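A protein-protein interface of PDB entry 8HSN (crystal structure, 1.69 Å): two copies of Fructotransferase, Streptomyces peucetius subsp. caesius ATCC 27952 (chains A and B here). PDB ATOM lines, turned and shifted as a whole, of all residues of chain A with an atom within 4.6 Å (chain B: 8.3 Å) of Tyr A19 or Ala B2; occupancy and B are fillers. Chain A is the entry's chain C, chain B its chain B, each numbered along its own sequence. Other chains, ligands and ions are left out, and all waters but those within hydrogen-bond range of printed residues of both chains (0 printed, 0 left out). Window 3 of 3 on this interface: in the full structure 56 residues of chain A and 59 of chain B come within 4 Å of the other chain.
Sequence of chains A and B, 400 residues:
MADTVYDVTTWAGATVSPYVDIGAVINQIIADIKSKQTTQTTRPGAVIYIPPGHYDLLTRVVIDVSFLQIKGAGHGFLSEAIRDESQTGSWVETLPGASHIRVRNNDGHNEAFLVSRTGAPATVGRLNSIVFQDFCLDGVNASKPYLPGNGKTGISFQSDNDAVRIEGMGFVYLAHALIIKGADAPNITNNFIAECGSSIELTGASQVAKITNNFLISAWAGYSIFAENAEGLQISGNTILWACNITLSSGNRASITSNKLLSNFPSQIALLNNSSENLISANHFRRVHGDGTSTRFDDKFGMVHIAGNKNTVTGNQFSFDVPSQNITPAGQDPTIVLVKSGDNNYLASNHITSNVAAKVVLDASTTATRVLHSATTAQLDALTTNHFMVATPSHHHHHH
N of Ala B2 is in hydrogen-bond range of OG1 of Thr A9, at 2.9 Å.
Printed residues of chain B that touch a printed residue of chain A: Ala B2, Thr B4, Val B5 and Pro B44.
Hydrophobic or aromatic side chains of chain B within 4 Å of the printed part of chain A: Ala B2, Val B5 and Pro B44.
Hydrophobic or aromatic side chains of chain A that line the printed part of chain B: Tyr A19, Pro A51 and His A54.
Along chain A the printed residues that touch a printed residue of chain B span positions 9 to 54.
Among the printed residues, merely in contact across the chains: Thr A10 with Ala B2, Tyr A19 with Ala B2, Pro A51 with Ala B2, Pro A51 with Thr B4, Pro A51 with Val B5 and His A54 with Pro B44.
Of the printed residues of chain A, Ala B2 touches Thr A9, Thr A10, Tyr A19 and Pro A51.
No residue of chain B comes within 4 Å of Pro A18.
Printed residues of chain A within 4 Å of Pro B44: His A54 (3.7 Å).
Printed residues of chain B within 4 Å of Pro A51: Ala B2, Thr B4 and Val B5.
Printed residues of chain A within 4 Å of Thr B4: Pro A51.
Printed residues of chain B within 4 Å of His A54: Pro B44 (3.7 Å).
Of the printed residues of chain A, Val B5 touches Pro A51 (3.9 Å).
The nearest residue of chain B that does not touch Tyr A19 is Asp B3 (5.7 Å).
The nearest printed residue of chain A that does not touch Ala B2 is Tyr A55 (4.9 Å).
No position is printed for both chains.
Of the 7 pairs that touch across the chains among the printed residues, none has its exchanged pair printed and touching as well.
O of Tyr A19 sits at hydrogen-bond distance from N of Asp A56.
The backbone carbonyl oxygen (O) of Pro A51 is in hydrogen-bond range of the side-chain hydroxyl (OH) of Tyr A55, at 2.7 Å.
The side-chain hydroxyl (OG) of Ser A17 is in hydrogen-bond range of the backbone NH (N) of Tyr A19 (3.1 Å).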
ATOM      1  N   THR A   9      21.650   3.852  -7.740  1.00  0.00           N
ATOM      2  CA  THR A   9      20.657   3.536  -8.766  1.00  0.00           C
ATOM      3  C   THR A   9      19.218   3.650  -8.294  1.00  0.00           C
ATOM      4  O   THR A   9      18.306   3.562  -9.128  1.00  0.00           O
ATOM      5  CB  THR A   9      20.860   2.120  -9.325  1.00  0.00           C
ATOM      6  OG1 THR A   9      20.465   1.147  -8.351  1.00  0.00           O
ATOM      7  CG2 THR A   9      22.291   1.900  -9.740  1.00  0.00           C
ATOM      8  N   THR A  10      18.978   3.821  -7.001  1.00  0.00           N
ATOM      9  CA  THR A  10      17.616   3.951  -6.501  1.00  0.00           C
ATOM     10  C   THR A  10      17.327   5.281  -5.826  1.00  0.00           C
ATOM     11  O   THR A  10      16.152   5.585  -5.574  1.00  0.00           O
ATOM     12  CB  THR A  10      17.295   2.829  -5.501  1.00  0.00           C
ATOM     13  OG1 THR A  10      18.053   3.033  -4.315  1.00  0.00           O
ATOM     14  CG2 THR A  10      17.592   1.484  -6.091  1.00  0.00           C
ATOM     15  N   SER A  17      21.343  10.193 -14.538  1.00  0.00           N
ATOM     16  CA  SER A  17      21.488   8.759 -14.376  1.00  0.00           C
ATOM     17  C   SER A  17      22.897   8.444 -13.897  1.00  0.00           C
ATOM     18  O   SER A  17      23.860   8.982 -14.451  1.00  0.00           O
ATOM     19  CB  SER A  17      21.262   8.047 -15.699  1.00  0.00           C
ATOM     20  OG  SER A  17      21.656   6.691 -15.591  1.00  0.00           O
ATOM     21  N   PRO A  18      23.061   7.551 -12.913  1.00  0.00           N
ATOM     22  CA  PRO A  18      24.430   7.166 -12.520  1.00  0.00           C
ATOM     23  C   PRO A  18      25.164   6.383 -13.593  1.00  0.00           C
ATOM     24  O   PRO A  18      26.402   6.312 -13.568  1.00  0.00           O
ATOM     25  CB  PRO A  18      24.215   6.317 -11.259  1.00  0.00           C
ATOM     26  CG  PRO A  18      22.881   5.683 -11.491  1.00  0.00           C
ATOM     27  CD  PRO A  18      22.038   6.727 -12.241  1.00  0.00           C
ATOM     28  N   TYR A  19      24.447   5.736 -14.511  1.00  0.00           N
ATOM     29  CA  TYR A  19      25.115   5.070 -15.617  1.00  0.00           C
ATOM     30  C   TYR A  19      25.746   6.084 -16.563  1.00  0.00           C
ATOM     31  O   TYR A  19      26.778   5.799 -17.182  1.00  0.00           O
ATOM     32  CB  TYR A  19      24.118   4.169 -16.353  1.00  0.00           C
ATOM     33  CG  TYR A  19      23.518   3.141 -15.442  1.00  0.00           C
ATOM     34  CD1 TYR A  19      24.236   2.018 -15.070  1.00  0.00           C
ATOM     35  CD2 TYR A  19      22.241   3.303 -14.915  1.00  0.00           C
ATOM     36  CE1 TYR A  19      23.702   1.073 -14.211  1.00  0.00           C
ATOM     37  CE2 TYR A  19      21.697   2.363 -14.055  1.00  0.00           C
ATOM     38  CZ  TYR A  19      22.427   1.251 -13.710  1.00  0.00           C
ATOM     39  OH  TYR A  19      21.893   0.306 -12.857  1.00  0.00           O
ATOM     40  N   VAL A  20      25.147   7.278 -16.657  1.00  0.00           N
ATOM     41  CA  VAL A  20      25.660   8.330 -17.533  1.00  0.00           C
ATOM     42  C   VAL A  20      26.768   9.116 -16.844  1.00  0.00           C
ATOM     43  O   VAL A  20      27.811   9.398 -17.448  1.00  0.00           O
ATOM     44  CB  VAL A  20      24.520   9.255 -17.983  1.00  0.00           C
ATOM     45  CG1 VAL A  20      25.075  10.422 -18.786  1.00  0.00           C
ATOM     46  CG2 VAL A  20      23.530   8.474 -18.810  1.00  0.00           C
ATOM     47  N   ASP A  21      26.550   9.512 -15.581  1.00  0.00           N
ATOM     48  CA  ASP A  21      27.587  10.217 -14.824  1.00  0.00           C
ATOM     49  C   ASP A  21      27.415   9.922 -13.329  1.00  0.00           C
ATOM     50  O   ASP A  21      26.780  10.683 -12.596  1.00  0.00           O
ATOM     51  CB  ASP A  21      27.524  11.710 -15.116  1.00  0.00           C
ATOM     52  CG  ASP A  21      28.642  12.495 -14.463  1.00  0.00           C
ATOM     53  OD1 ASP A  21      29.513  11.902 -13.778  1.00  0.00           O
ATOM     54  OD2 ASP A  21      28.633  13.740 -14.598  1.00  0.00           O
ATOM     55  N   PRO A  51      25.627  -0.890  -6.948  1.00  0.00           N
ATOM     56  CA  PRO A  51      25.350  -2.273  -7.378  1.00  0.00           C
ATOM     57  C   PRO A  51      26.180  -2.634  -8.596  1.00  0.00           C
ATOM     58  O   PRO A  51      26.734  -1.750  -9.264  1.00  0.00           O
ATOM     59  CB  PRO A  51      23.847  -2.257  -7.729  1.00  0.00           C
ATOM     60  CG  PRO A  51      23.339  -0.939  -7.371  1.00  0.00           C
ATOM     61  CD  PRO A  51      24.471   0.007  -7.157  1.00  0.00           C
ATOM     62  N   HIS A  54      27.808  -1.093 -15.243  1.00  0.00           N
ATOM     63  CA  HIS A  54      28.785  -0.248 -15.931  1.00  0.00           C
ATOM     64  C   HIS A  54      28.363   1.208 -15.797  1.00  0.00           C
ATOM     65  O   HIS A  54      27.331   1.614 -16.357  1.00  0.00           O
ATOM     66  CB  HIS A  54      28.880  -0.597 -17.416  1.00  0.00           C
ATOM     67  CG  HIS A  54      29.439  -1.955 -17.709  1.00  0.00           C
ATOM     68  ND1 HIS A  54      30.632  -2.409 -17.180  1.00  0.00           N
ATOM     69  CD2 HIS A  54      28.989  -2.939 -18.521  1.00  0.00           C
ATOM     70  CE1 HIS A  54      30.873  -3.625 -17.640  1.00  0.00           C
ATOM     71  NE2 HIS A  54      29.889  -3.970 -18.455  1.00  0.00           N
ATOM     72  N   TYR A  55      29.170   2.001 -15.096  1.00  0.00           N
ATOM     73  CA  TYR A  55      28.860   3.395 -14.830  1.00  0.00           C
ATOM     74  C   TYR A  55      29.944   4.293 -15.398  1.00  0.00           C
ATOM     75  O   TYR A  55      31.123   4.128 -15.069  1.00  0.00           O
ATOM     76  CB  TYR A  55      28.747   3.668 -13.325  1.00  0.00           C
ATOM     77  CG  TYR A  55      27.827   2.734 -12.585  1.00  0.00           C
ATOM     78  CD1 TYR A  55      28.277   1.505 -12.096  1.00  0.00           C
ATOM     79  CD2 TYR A  55      26.509   3.089 -12.337  1.00  0.00           C
ATOM     80  CE1 TYR A  55      27.420   0.656 -11.392  1.00  0.00           C
ATOM     81  CE2 TYR A  55      25.657   2.248 -11.641  1.00  0.00           C
ATOM     82  CZ  TYR A  55      26.114   1.034 -11.175  1.00  0.00           C
ATOM     83  OH  TYR A  55      25.246   0.205 -10.469  1.00  0.00           O
ATOM     84  N   ASP A  56      29.557   5.257 -16.225  1.00  0.00           N
ATOM     85  CA  ASP A  56      30.497   6.291 -16.629  1.00  0.00           C
ATOM     86  C   ASP A  56      30.595   7.344 -15.538  1.00  0.00           C
ATOM     87  O   ASP A  56      29.582   7.758 -14.969  1.00  0.00           O
ATOM     88  CB  ASP A  56      30.055   6.979 -17.926  1.00  0.00           C
ATOM     89  CG  ASP A  56      30.377   6.170 -19.173  1.00  0.00           C
ATOM     90  OD1 ASP A  56      30.894   5.048 -19.056  1.00  0.00           O
ATOM     91  OD2 ASP A  56      30.089   6.664 -20.293  1.00  0.00           O
ATOM     92  N   ALA B   2      18.934  -1.321  -8.600  1.00  0.00           N
ATOM     93  CA  ALA B   2      19.308  -1.956  -9.859  1.00  0.00           C
ATOM     94  C   ALA B   2      18.822  -3.397  -9.866  1.00  0.00           C
ATOM     95  O   ALA B   2      18.640  -3.993  -8.818  1.00  0.00           O
ATOM     96  CB  ALA B   2      20.812  -1.914 -10.058  1.00  0.00           C
ATOM     97  N   ASP B   3      18.703  -3.995 -11.045  1.00  0.00           N
ATOM     98  CA  ASP B   3      18.224  -5.365 -11.135  1.00  0.00           C
ATOM     99  C   ASP B   3      19.359  -6.395 -11.088  1.00  0.00           C
ATOM    100  O   ASP B   3      19.127  -7.570 -11.365  1.00  0.00           O
ATOM    101  CB  ASP B   3      17.363  -5.539 -12.395  1.00  0.00           C
ATOM    102  CG  ASP B   3      18.144  -5.443 -13.680  1.00  0.00           C
ATOM    103  OD1 ASP B   3      19.396  -5.398 -13.653  1.00  0.00           O
ATOM    104  OD2 ASP B   3      17.492  -5.426 -14.753  1.00  0.00           O
ATOM    105  N   THR B   4      20.555  -5.990 -10.672  1.00  0.00           N
ATOM    106  CA  THR B   4      21.706  -6.872 -10.574  1.00  0.00           C
ATOM    107  C   THR B   4      21.925  -7.419  -9.164  1.00  0.00           C
ATOM    108  O   THR B   4      22.965  -8.045  -8.910  1.00  0.00           O
ATOM    109  CB  THR B   4      22.959  -6.119 -11.004  1.00  0.00           C
ATOM    110  OG1 THR B   4      23.036  -4.900 -10.247  1.00  0.00           O
ATOM    111  CG2 THR B   4      22.922  -5.795 -12.509  1.00  0.00           C
ATOM    112  N   VAL B   5      20.994  -7.181  -8.246  1.00  0.00           N
ATOM    113  CA  VAL B   5      21.106  -7.630  -6.867  1.00  0.00           C
ATOM    114  C   VAL B   5      19.968  -8.590  -6.584  1.00  0.00           C
ATOM    115  O   VAL B   5      18.793  -8.222  -6.715  1.00  0.00           O
ATOM    116  CB  VAL B   5      21.080  -6.452  -5.885  1.00  0.00           C
ATOM    117  CG1 VAL B   5      21.101  -6.982  -4.469  1.00  0.00           C
ATOM    118  CG2 VAL B   5      22.256  -5.512  -6.158  1.00  0.00           C
ATOM    119  N   TYR B   6      20.312  -9.810  -6.192  1.00  0.00           N
ATOM    120  CA  TYR B   6      19.352 -10.851  -5.871  1.00  0.00           C
ATOM    121  C   TYR B   6      19.542 -11.280  -4.426  1.00  0.00           C
ATOM    122  O   TYR B   6      20.657 -11.256  -3.900  1.00  0.00           O
ATOM    123  CB  TYR B   6      19.527 -12.090  -6.742  1.00  0.00           C
ATOM    124  CG  TYR B   6      19.406 -11.886  -8.248  1.00  0.00           C
ATOM    125  CD1 TYR B   6      20.437 -11.326  -8.977  1.00  0.00           C
ATOM    126  CD2 TYR B   6      18.270 -12.299  -8.931  1.00  0.00           C
ATOM    127  CE1 TYR B   6      20.357 -11.172 -10.338  1.00  0.00           C
ATOM    128  CE2 TYR B   6      18.171 -12.134 -10.297  1.00  0.00           C
ATOM    129  CZ  TYR B   6      19.214 -11.568 -10.994  1.00  0.00           C
ATOM    130  OH  TYR B   6      19.135 -11.394 -12.361  1.00  0.00           O
ATOM    131  N   PRO B  44      28.296  -6.827 -16.708  1.00  0.00           N
ATOM    132  CA  PRO B  44      28.977  -6.433 -15.464  1.00  0.00           C
ATOM    133  C   PRO B  44      28.851  -7.442 -14.334  1.00  0.00           C
ATOM    134  O   PRO B  44      29.635  -7.365 -13.385  1.00  0.00           O
ATOM    135  CB  PRO B  44      28.288  -5.117 -15.087  1.00  0.00           C
ATOM    136  CG  PRO B  44      26.894  -5.244 -15.699  1.00  0.00           C
ATOM    137  CD  PRO B  44      27.124  -5.968 -16.993  1.00  0.00           C
